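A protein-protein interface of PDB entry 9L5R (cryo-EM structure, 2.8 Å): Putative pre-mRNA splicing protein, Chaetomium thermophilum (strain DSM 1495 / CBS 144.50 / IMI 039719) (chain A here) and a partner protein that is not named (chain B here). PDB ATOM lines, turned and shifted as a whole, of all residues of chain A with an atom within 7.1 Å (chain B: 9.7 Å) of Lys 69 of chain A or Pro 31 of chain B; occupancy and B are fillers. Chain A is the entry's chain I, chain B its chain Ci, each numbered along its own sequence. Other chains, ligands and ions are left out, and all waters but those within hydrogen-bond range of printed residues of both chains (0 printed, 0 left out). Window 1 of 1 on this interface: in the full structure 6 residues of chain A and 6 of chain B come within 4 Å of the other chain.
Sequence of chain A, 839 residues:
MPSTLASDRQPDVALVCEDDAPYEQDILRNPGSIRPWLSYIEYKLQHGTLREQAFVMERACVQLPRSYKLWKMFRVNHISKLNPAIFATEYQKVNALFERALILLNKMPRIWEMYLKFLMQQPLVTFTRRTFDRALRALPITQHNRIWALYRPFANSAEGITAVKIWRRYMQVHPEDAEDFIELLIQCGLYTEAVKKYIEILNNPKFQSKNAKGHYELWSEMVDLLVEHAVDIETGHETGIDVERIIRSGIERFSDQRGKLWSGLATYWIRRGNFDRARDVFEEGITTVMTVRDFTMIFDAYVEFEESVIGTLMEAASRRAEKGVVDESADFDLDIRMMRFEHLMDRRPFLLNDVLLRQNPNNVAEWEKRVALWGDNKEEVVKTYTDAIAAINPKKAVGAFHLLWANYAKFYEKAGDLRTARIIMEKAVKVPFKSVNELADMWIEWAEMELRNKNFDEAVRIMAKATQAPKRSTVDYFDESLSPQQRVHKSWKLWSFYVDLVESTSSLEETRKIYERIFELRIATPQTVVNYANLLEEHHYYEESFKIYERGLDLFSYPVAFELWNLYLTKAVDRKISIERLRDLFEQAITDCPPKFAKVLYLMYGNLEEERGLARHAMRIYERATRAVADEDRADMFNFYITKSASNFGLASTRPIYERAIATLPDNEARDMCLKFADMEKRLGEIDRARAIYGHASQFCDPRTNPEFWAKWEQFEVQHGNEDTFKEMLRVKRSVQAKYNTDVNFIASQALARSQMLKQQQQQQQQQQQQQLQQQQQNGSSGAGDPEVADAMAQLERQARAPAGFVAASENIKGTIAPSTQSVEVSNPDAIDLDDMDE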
ATOM      1  N   ILE A  34       9.515   2.725  -1.583  1.00  0.00           N
ATOM      2  CA  ILE A  34       9.793   2.728  -0.152  1.00  0.00           C
ATOM      3  C   ILE A  34       9.086   1.589   0.580  1.00  0.00           C
ATOM      4  O   ILE A  34       9.449   1.281   1.724  1.00  0.00           O
ATOM      5  CB  ILE A  34       9.408   4.097   0.449  1.00  0.00           C
ATOM      6  CG1 ILE A  34      10.201   4.388   1.728  1.00  0.00           C
ATOM      7  CG2 ILE A  34       7.907   4.183   0.707  1.00  0.00           C
ATOM      8  CD1 ILE A  34       9.873   5.725   2.359  1.00  0.00           C
ATOM      9  N   LEU A  38      10.324  -0.462   3.851  1.00  0.00           N
ATOM     10  CA  LEU A  38       9.540  -0.370   5.080  1.00  0.00           C
ATOM     11  C   LEU A  38       9.207  -1.752   5.628  1.00  0.00           C
ATOM     12  O   LEU A  38       9.305  -1.986   6.838  1.00  0.00           O
ATOM     13  CB  LEU A  38       8.260   0.427   4.832  1.00  0.00           C
ATOM     14  CG  LEU A  38       8.378   1.953   4.793  1.00  0.00           C
ATOM     15  CD1 LEU A  38       7.099   2.572   4.252  1.00  0.00           C
ATOM     16  CD2 LEU A  38       8.697   2.502   6.175  1.00  0.00           C
ATOM     17  N   ARG A  66      17.537  10.352  -0.040  1.00  0.00           N
ATOM     18  CA  ARG A  66      16.514  11.385   0.040  1.00  0.00           C
ATOM     19  C   ARG A  66      15.305  10.952   0.857  1.00  0.00           C
ATOM     20  O   ARG A  66      14.364  11.739   1.007  1.00  0.00           O
ATOM     21  CB  ARG A  66      16.059  11.796  -1.365  1.00  0.00           C
ATOM     22  CG  ARG A  66      17.079  12.610  -2.143  1.00  0.00           C
ATOM     23  CD  ARG A  66      16.479  13.158  -3.428  1.00  0.00           C
ATOM     24  NE  ARG A  66      17.404  14.040  -4.129  1.00  0.00           N
ATOM     25  CZ  ARG A  66      17.109  14.710  -5.235  1.00  0.00           C
ATOM     26  NH1 ARG A  66      15.915  14.622  -5.799  1.00  0.00           N
ATOM     27  NH2 ARG A  66      18.034  15.488  -5.789  1.00  0.00           N
ATOM     28  N   SER A  67      15.306   9.730   1.381  1.00  0.00           N
ATOM     29  CA  SER A  67      14.170   9.198   2.130  1.00  0.00           C
ATOM     30  C   SER A  67      14.265   9.700   3.565  1.00  0.00           C
ATOM     31  O   SER A  67      14.880   9.057   4.426  1.00  0.00           O
ATOM     32  CB  SER A  67      14.144   7.677   2.061  1.00  0.00           C
ATOM     33  OG  SER A  67      12.898   7.178   2.506  1.00  0.00           O
ATOM     34  N   TYR A  68      13.643  10.858   3.817  1.00  0.00           N
ATOM     35  CA  TYR A  68      13.654  11.457   5.148  1.00  0.00           C
ATOM     36  C   TYR A  68      12.961  10.572   6.173  1.00  0.00           C
ATOM     37  O   TYR A  68      13.400  10.509   7.323  1.00  0.00           O
ATOM     38  CB  TYR A  68      13.001  12.841   5.102  1.00  0.00           C
ATOM     39  CG  TYR A  68      12.566  13.383   6.448  1.00  0.00           C
ATOM     40  CD1 TYR A  68      13.496  13.845   7.371  1.00  0.00           C
ATOM     41  CD2 TYR A  68      11.218  13.440   6.791  1.00  0.00           C
ATOM     42  CE1 TYR A  68      13.098  14.343   8.602  1.00  0.00           C
ATOM     43  CE2 TYR A  68      10.811  13.936   8.017  1.00  0.00           C
ATOM     44  CZ  TYR A  68      11.754  14.385   8.918  1.00  0.00           C
ATOM     45  OH  TYR A  68      11.352  14.879  10.138  1.00  0.00           O
ATOM     46  N   LYS A  69      11.903   9.864   5.773  1.00  0.00           N
ATOM     47  CA  LYS A  69      11.200   8.977   6.696  1.00  0.00           C
ATOM     48  C   LYS A  69      12.077   7.801   7.118  1.00  0.00           C
ATOM     49  O   LYS A  69      12.200   7.503   8.314  1.00  0.00           O
ATOM     50  CB  LYS A  69       9.905   8.482   6.049  1.00  0.00           C
ATOM     51  CG  LYS A  69       8.882   7.929   7.020  1.00  0.00           C
ATOM     52  CD  LYS A  69       7.634   7.462   6.290  1.00  0.00           C
ATOM     53  CE  LYS A  69       6.552   7.032   7.265  1.00  0.00           C
ATOM     54  NZ  LYS A  69       5.231   6.872   6.598  1.00  0.00           N
ATOM     55  N   LEU A  70      12.704   7.129   6.144  1.00  0.00           N
ATOM     56  CA  LEU A  70      13.565   5.989   6.458  1.00  0.00           C
ATOM     57  C   LEU A  70      14.776   6.417   7.275  1.00  0.00           C
ATOM     58  O   LEU A  70      15.170   5.724   8.223  1.00  0.00           O
ATOM     59  CB  LEU A  70      14.007   5.278   5.177  1.00  0.00           C
ATOM     60  CG  LEU A  70      12.949   4.516   4.374  1.00  0.00           C
ATOM     61  CD1 LEU A  70      13.586   3.807   3.185  1.00  0.00           C
ATOM     62  CD2 LEU A  70      12.190   3.532   5.249  1.00  0.00           C
ATOM     63  N   TRP A  71      15.366   7.571   6.947  1.00  0.00           N
ATOM     64  CA  TRP A  71      16.464   8.057   7.776  1.00  0.00           C
ATOM     65  C   TRP A  71      15.973   8.502   9.155  1.00  0.00           C
ATOM     66  O   TRP A  71      16.733   8.448  10.124  1.00  0.00           O
ATOM     67  CB  TRP A  71      17.213   9.191   7.074  1.00  0.00           C
ATOM     68  CG  TRP A  71      18.365   9.682   7.889  1.00  0.00           C
ATOM     69  CD1 TRP A  71      19.618   9.147   7.949  1.00  0.00           C
ATOM     70  CD2 TRP A  71      18.353  10.779   8.807  1.00  0.00           C
ATOM     71  NE1 TRP A  71      20.394   9.856   8.832  1.00  0.00           N
ATOM     72  CE2 TRP A  71      19.637  10.861   9.377  1.00  0.00           C
ATOM     73  CE3 TRP A  71      17.381  11.701   9.199  1.00  0.00           C
ATOM     74  CZ2 TRP A  71      19.977  11.835  10.311  1.00  0.00           C
ATOM     75  CZ3 TRP A  71      17.718  12.663  10.125  1.00  0.00           C
ATOM     76  CH2 TRP A  71      19.004  12.726  10.670  1.00  0.00           C
ATOM     77  N   LYS A  72      14.707   8.923   9.269  1.00  0.00           N
ATOM     78  CA  LYS A  72      14.150   9.252  10.579  1.00  0.00           C
ATOM     79  C   LYS A  72      14.013   8.014  11.454  1.00  0.00           C
ATOM     80  O   LYS A  72      14.342   8.055  12.645  1.00  0.00           O
ATOM     81  CB  LYS A  72      12.796   9.944  10.422  1.00  0.00           C
ATOM     82  CG  LYS A  72      12.216  10.479  11.725  1.00  0.00           C
ATOM     83  CD  LYS A  72      10.878  11.163  11.487  1.00  0.00           C
ATOM     84  CE  LYS A  72      10.289  11.714  12.776  1.00  0.00           C
ATOM     85  NZ  LYS A  72       8.934  12.293  12.548  1.00  0.00           N
ATOM     86  N   MET A  73      13.527   6.901  10.893  1.00  0.00           N
ATOM     87  CA  MET A  73      13.533   5.661  11.673  1.00  0.00           C
ATOM     88  C   MET A  73      14.956   5.205  11.985  1.00  0.00           C
ATOM     89  O   MET A  73      15.212   4.669  13.071  1.00  0.00           O
ATOM     90  CB  MET A  73      12.751   4.519  11.008  1.00  0.00           C
ATOM     91  CG  MET A  73      11.218   4.579  11.115  1.00  0.00           C
ATOM     92  SD  MET A  73      10.265   5.742  10.137  1.00  0.00           S
ATOM     93  CE  MET A  73      10.381   4.920   8.547  1.00  0.00           C
ATOM     94  N   PHE A  74      15.895   5.421  11.055  1.00  0.00           N
ATOM     95  CA  PHE A  74      17.294   5.083  11.316  1.00  0.00           C
ATOM     96  C   PHE A  74      17.857   5.874  12.494  1.00  0.00           C
ATOM     97  O   PHE A  74      18.492   5.300  13.388  1.00  0.00           O
ATOM     98  CB  PHE A  74      18.129   5.324  10.057  1.00  0.00           C
ATOM     99  CG  PHE A  74      19.614   5.239  10.280  1.00  0.00           C
ATOM    100  CD1 PHE A  74      20.189   4.117  10.862  1.00  0.00           C
ATOM    101  CD2 PHE A  74      20.438   6.284   9.897  1.00  0.00           C
ATOM    102  CE1 PHE A  74      21.551   4.043  11.061  1.00  0.00           C
ATOM    103  CE2 PHE A  74      21.802   6.215  10.093  1.00  0.00           C
ATOM    104  CZ  PHE A  74      22.359   5.093  10.675  1.00  0.00           C
ATOM    105  N   ARG A  75      17.617   7.188  12.528  1.00  0.00           N
ATOM    106  CA  ARG A  75      18.139   7.994  13.627  1.00  0.00           C
ATOM    107  C   ARG A  75      17.399   7.716  14.930  1.00  0.00           C
ATOM    108  O   ARG A  75      18.010   7.779  16.000  1.00  0.00           O
ATOM    109  CB  ARG A  75      18.100   9.488  13.282  1.00  0.00           C
ATOM    110  CG  ARG A  75      16.717  10.108  13.167  1.00  0.00           C
ATOM    111  CD  ARG A  75      16.740  11.617  13.356  1.00  0.00           C
ATOM    112  NE  ARG A  75      16.909  12.014  14.749  1.00  0.00           N
ATOM    113  CZ  ARG A  75      15.912  12.154  15.611  1.00  0.00           C
ATOM    114  NH1 ARG A  75      14.657  11.923  15.260  1.00  0.00           N
ATOM    115  NH2 ARG A  75      16.179  12.543  16.855  1.00  0.00           N
ATOM    116  N   LEU A 105      20.241  16.268   2.351  1.00  0.00           N
ATOM    117  CA  LEU A 105      18.917  16.696   2.802  1.00  0.00           C
ATOM    118  C   LEU A 105      19.022  18.027   3.546  1.00  0.00           C
ATOM    119  O   LEU A 105      18.495  18.191   4.647  1.00  0.00           O
ATOM    120  CB  LEU A 105      18.264  15.630   3.682  1.00  0.00           C
ATOM    121  CG  LEU A 105      17.777  14.345   3.005  1.00  0.00           C
ATOM    122  CD1 LEU A 105      17.295  13.340   4.040  1.00  0.00           C
ATOM    123  CD2 LEU A 105      16.679  14.653   1.998  1.00  0.00           C
ATOM    124  N   VAL B  24       6.054  17.922  -9.385  1.00  0.00           N
ATOM    125  CA  VAL B  24       6.985  18.604  -8.488  1.00  0.00           C
ATOM    126  C   VAL B  24       6.541  18.457  -7.038  1.00  0.00           C
ATOM    127  O   VAL B  24       7.368  18.247  -6.141  1.00  0.00           O
ATOM    128  CB  VAL B  24       7.126  20.083  -8.891  1.00  0.00           C
ATOM    129  N   LEU B  25       5.232  18.563  -6.786  1.00  0.00           N
ATOM    130  CA  LEU B  25       4.715  18.381  -5.431  1.00  0.00           C
ATOM    131  C   LEU B  25       4.937  16.956  -4.936  1.00  0.00           C
ATOM    132  O   LEU B  25       5.291  16.746  -3.770  1.00  0.00           O
ATOM    133  CB  LEU B  25       3.229  18.739  -5.386  1.00  0.00           C
ATOM    134  N   HIS B  26       4.740  15.967  -5.812  1.00  0.00           N
ATOM    135  CA  HIS B  26       4.982  14.576  -5.440  1.00  0.00           C
ATOM    136  C   HIS B  26       6.461  14.319  -5.173  1.00  0.00           C
ATOM    137  O   HIS B  26       6.809  13.589  -4.239  1.00  0.00           O
ATOM    138  CB  HIS B  26       4.463  13.642  -6.532  1.00  0.00           C
ATOM    139  N   GLU B  27       7.345  14.915  -5.980  1.00  0.00           N
ATOM    140  CA  GLU B  27       8.779  14.762  -5.754  1.00  0.00           C
ATOM    141  C   GLU B  27       9.210  15.432  -4.454  1.00  0.00           C
ATOM    142  O   GLU B  27      10.119  14.945  -3.771  1.00  0.00           O
ATOM    143  CB  GLU B  27       9.560  15.332  -6.938  1.00  0.00           C
ATOM    144  N   ALA B  28       8.577  16.553  -4.102  1.00  0.00           N
ATOM    145  CA  ALA B  28       8.887  17.209  -2.838  1.00  0.00           C
ATOM    146  C   ALA B  28       8.371  16.405  -1.648  1.00  0.00           C
ATOM    147  O   ALA B  28       9.043  16.318  -0.615  1.00  0.00           O
ATOM    148  CB  ALA B  28       8.306  18.622  -2.823  1.00  0.00           C
ATOM    149  N   PHE B  29       7.185  15.811  -1.774  1.00  0.00           N
ATOM    150  CA  PHE B  29       6.558  15.094  -0.671  1.00  0.00           C
ATOM    151  C   PHE B  29       6.994  13.637  -0.568  1.00  0.00           C
ATOM    152  O   PHE B  29       6.637  12.972   0.411  1.00  0.00           O
ATOM    153  CB  PHE B  29       5.033  15.162  -0.801  1.00  0.00           C
ATOM    154  N   LEU B  30       7.740  13.123  -1.547  1.00  0.00           N
ATOM    155  CA  LEU B  30       8.210  11.743  -1.513  1.00  0.00           C
ATOM    156  C   LEU B  30       9.233  11.529  -0.404  1.00  0.00           C
ATOM    157  O   LEU B  30       9.359  10.410   0.111  1.00  0.00           O
ATOM    158  CB  LEU B  30       8.812  11.355  -2.865  1.00  0.00           C
ATOM    159  N   PRO B  31      10.001  12.559  -0.036  1.00  0.00           N
ATOM    160  CA  PRO B  31      10.966  12.392   1.065  1.00  0.00           C
ATOM    161  C   PRO B  31      10.317  12.097   2.407  1.00  0.00           C
ATOM    162  O   PRO B  31      10.848  11.287   3.176  1.00  0.00           O
ATOM    163  CB  PRO B  31      11.709  13.734   1.081  1.00  0.00           C
ATOM    164  N   PHE B  32       9.174  12.717   2.707  1.00  0.00           N
ATOM    165  CA  PHE B  32       8.485  12.457   3.963  1.00  0.00           C
ATOM    166  C   PHE B  32       7.756  11.121   3.966  1.00  0.00           C
ATOM    167  O   PHE B  32       7.455  10.596   5.043  1.00  0.00           O
ATOM    168  CB  PHE B  32       7.494  13.584   4.265  1.00  0.00           C
ATOM    169  N   GLY B  33       7.469  10.569   2.802  1.00  0.00           N
ATOM    170  CA  GLY B  33       6.769   9.305   2.709  1.00  0.00           C
ATOM    171  C   GLY B  33       6.008   9.219   1.403  1.00  0.00           C
ATOM    172  O   GLY B  33       6.066  10.110   0.560  1.00  0.00           O
ATOM    173  N   GLU B  34       5.288   8.111   1.254  1.00  0.00           N
ATOM    174  CA  GLU B  34       4.484   7.902   0.059  1.00  0.00           C
ATOM    175  C   GLU B  34       3.251   8.796   0.083  1.00  0.00           C
ATOM    176  O   GLU B  34       2.562   8.906   1.101  1.00  0.00           O
ATOM    177  CB  GLU B  34       4.069   6.436  -0.053  1.00  0.00           C
ATOM    178  N   ILE B  35       2.976   9.436  -1.048  1.00  0.00           N
ATOM    179  CA  ILE B  35       1.811  10.301  -1.205  1.00  0.00           C
ATOM    180  C   ILE B  35       0.745   9.517  -1.957  1.00  0.00           C
ATOM    181  O   ILE B  35       0.977   9.060  -3.083  1.00  0.00           O
ATOM    182  CB  ILE B  35       2.169  11.600  -1.942  1.00  0.00           C
ATOM    183  N   PHE B  62      -1.159  11.630   1.908  1.00  0.00           N
ATOM    184  CA  PHE B  62      -0.133  10.621   2.110  1.00  0.00           C
ATOM    185  C   PHE B  62      -0.756   9.314   2.589  1.00  0.00           C
ATOM    186  O   PHE B  62      -1.937   9.244   2.937  1.00  0.00           O
ATOM    187  CB  PHE B  62       0.916  11.115   3.112  1.00  0.00           C
ATOM    188  N   GLU B  63       0.067   8.263   2.600  1.00  0.00           N
ATOM    189  CA  GLU B  63      -0.415   6.953   3.021  1.00  0.00           C
ATOM    190  C   GLU B  63      -0.598   6.872   4.532  1.00  0.00           C
ATOM    191  O   GLU B  63      -1.447   6.112   5.010  1.00  0.00           O
ATOM    192  CB  GLU B  63       0.547   5.862   2.545  1.00  0.00           C
ATOM    193  N   ASP B  64       0.180   7.640   5.295  1.00  0.00           N
ATOM    194  CA  ASP B  64       0.105   7.576   6.742  1.00  0.00           C
ATOM    195  C   ASP B  64      -0.111   8.962   7.337  1.00  0.00           C
ATOM    196  O   ASP B  64       0.383   9.956   6.789  1.00  0.00           O
ATOM    197  CB  ASP B  64       1.383   6.962   7.333  1.00  0.00           C
ATOM    198  N   PRO B  65      -0.861   9.063   8.439  1.00  0.00           N
ATOM    199  CA  PRO B  65      -0.988  10.362   9.121  1.00  0.00           C
ATOM    200  C   PRO B  65       0.328  10.890   9.665  1.00  0.00           C
ATOM    201  O   PRO B  65       0.536  12.109   9.677  1.00  0.00           O
ATOM    202  CB  PRO B  65      -1.990  10.067  10.245  1.00  0.00           C
ATOM    203  N   GLU B  66       1.225  10.005  10.111  1.00  0.00           N
ATOM    204  CA  GLU B  66       2.547  10.442  10.549  1.00  0.00           C
ATOM    205  C   GLU B  66       3.354  11.011   9.387  1.00  0.00           C
ATOM    206  O   GLU B  66       4.044  12.026   9.542  1.00  0.00           O
ATOM    207  CB  GLU B  66       3.294   9.280  11.204  1.00  0.00           C
ATOM    208  N   ASP B  67       3.271  10.374   8.216  1.00  0.00           N
ATOM    209  CA  ASP B  67       3.937  10.900   7.028  1.00  0.00           C
ATOM    210  C   ASP B  67       3.333  12.233   6.600  1.00  0.00           C
ATOM    211  O   ASP B  67       4.057  13.135   6.165  1.00  0.00           O
ATOM    212  CB  ASP B  67       3.858   9.886   5.888  1.00  0.00           C
ATOM    213  N   ALA B  68       2.010  12.372   6.721  1.00  0.00           N
ATOM    214  CA  ALA B  68       1.359  13.640   6.399  1.00  0.00           C
ATOM    215  C   ALA B  68       1.794  14.747   7.353  1.00  0.00           C
ATOM    216  O   ALA B  68       2.030  15.883   6.927  1.00  0.00           O
ATOM    217  CB  ALA B  68      -0.159  13.473   6.429  1.00  0.00           C
ATOM    218  N   LYS B  69       1.910  14.433   8.647  1.00  0.00           N
ATOM    219  CA  LYS B  69       2.378  15.418   9.618  1.00  0.00           C
ATOM    220  C   LYS B  69       3.836  15.794   9.373  1.00  0.00           C
ATOM    221  O   LYS B  69       4.210  16.965   9.511  1.00  0.00           O
ATOM    222  CB  LYS B  69       2.195  14.883  11.038  1.00  0.00           C
ATOM    223  N   GLU B  70       4.670  14.815   9.008  1.00  0.00           N
ATOM    224  CA  GLU B  70       6.064  15.105   8.683  1.00  0.00           C
ATOM    225  C   GLU B  70       6.173  15.982   7.441  1.00  0.00           C
ATOM    226  O   GLU B  70       6.988  16.911   7.398  1.00  0.00           O
ATOM    227  CB  GLU B  70       6.839  13.801   8.490  1.00  0.00           C
ATOM    228  N   ALA B  71       5.351  15.708   6.423  1.00  0.00           N
ATOM    229  CA  ALA B  71       5.338  16.542   5.226  1.00  0.00           C
ATOM    230  C   ALA B  71       4.831  17.947   5.523  1.00  0.00           C
ATOM    231  O   ALA B  71       5.329  18.917   4.939  1.00  0.00           O
ATOM    232  CB  ALA B  71       4.485  15.889   4.139  1.00  0.00           C
ATOM    233  N   ILE B  72       3.843  18.073   6.413  1.00  0.00           N
ATOM    234  CA  ILE B  72       3.354  19.389   6.813  1.00  0.00           C
ATOM    235  C   ILE B  72       4.438  20.165   7.550  1.00  0.00           C
ATOM    236  O   ILE B  72       4.633  21.362   7.309  1.00  0.00           O
ATOM    237  CB  ILE B  72       2.080  19.247   7.666  1.00  0.00           C
ATOM    238  N   ASN B  74       7.612  19.727   7.184  1.00  0.00           N
ATOM    239  CA  ASN B  74       8.691  20.006   6.243  1.00  0.00           C
ATOM    240  C   ASN B  74       8.347  21.180   5.333  1.00  0.00           C
ATOM    241  O   ASN B  74       9.113  22.143   5.226  1.00  0.00           O
ATOM    242  CB  ASN B  74       8.997  18.756   5.412  1.00  0.00           C
ATOM    243  N   MET B  75       7.194  21.114   4.669  1.00  0.00           N
ATOM    244  CA  MET B  75       6.800  22.123   3.695  1.00  0.00           C
ATOM    245  C   MET B  75       6.099  23.323   4.317  1.00  0.00           C
ATOM    246  O   MET B  75       5.730  24.246   3.585  1.00  0.00           O
ATOM    247  CB  MET B  75       5.888  21.499   2.632  1.00  0.00           C
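CB of Pro 31 of chain B touches O of Arg 66 of chain A, at 3.3 Å.
Ser 67 of chain A touches Pro 31 of chain B (C to O, 3.8 Å).
CD of Lys 69 of chain A touches O of Phe 32 of chain B, at 3.4 Å.
Asp 64 of chain B touches Lys 69 of chain A.
NZ of Lys 69 of chain A touches CB of Asp 67 of chain B (3.4 Å).
Along chain A the printed residues that touch a printed residue of chain B span positions 66 to 69.
Of the 25 printed residues of chain B, 4 touch a printed residue of chain A.
Hydrophobic or aromatic side chains of chain B within 4 Å of the printed part of chain A: Pro 31.
Among the printed residues, 7 pairs touch across the chains.
Among the printed residues, no Asp or Glu carboxylate lies within 4 Å of a Lys or Arg side-chain nitrogen of the other chain.
Printed residues of chain B within 4 Å of Arg 66 of chain A: Pro 31 (3.3 Å).
Printed residues of chain B within 4 Å of Ser 67 of chain A: Pro 31 (3.8 Å).
Of the printed residues of chain B, Lys 69 of chain A touches Pro 31, Phe 32, Asp 64 and Asp 67.
Leu 70 of chain A touches none of the printed residues of chain B.
His 26 of chain B touches none of the printed residues of chain A.
Pro 31 of chain B touches four residues of chain A.
Of the printed residues of chain A, Phe 32 of chain B touches Lys 69.
Printed residues of chain A within 4 Å of Asp 64 of chain B: Lys 69 (3.9 Å).
The nearest residue of chain A that does not touch Pro 31 of chain B is Leu 105 of chain A (5.1 Å).
The nearest printed residue of chain B that does not touch Tyr 68 of chain A is Glu 70 of chain B (4.002 Å).
O of Pro 31 of chain B is in hydrogen-bond range of N of Lys 69 of chain A, 3.1 Å away.
The backbone NH (N) of Tyr 68 of chain A is in hydrogen-bond range of the backbone carbonyl oxygen (O) of Pro 31 of chain B, at 2.9 Å.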
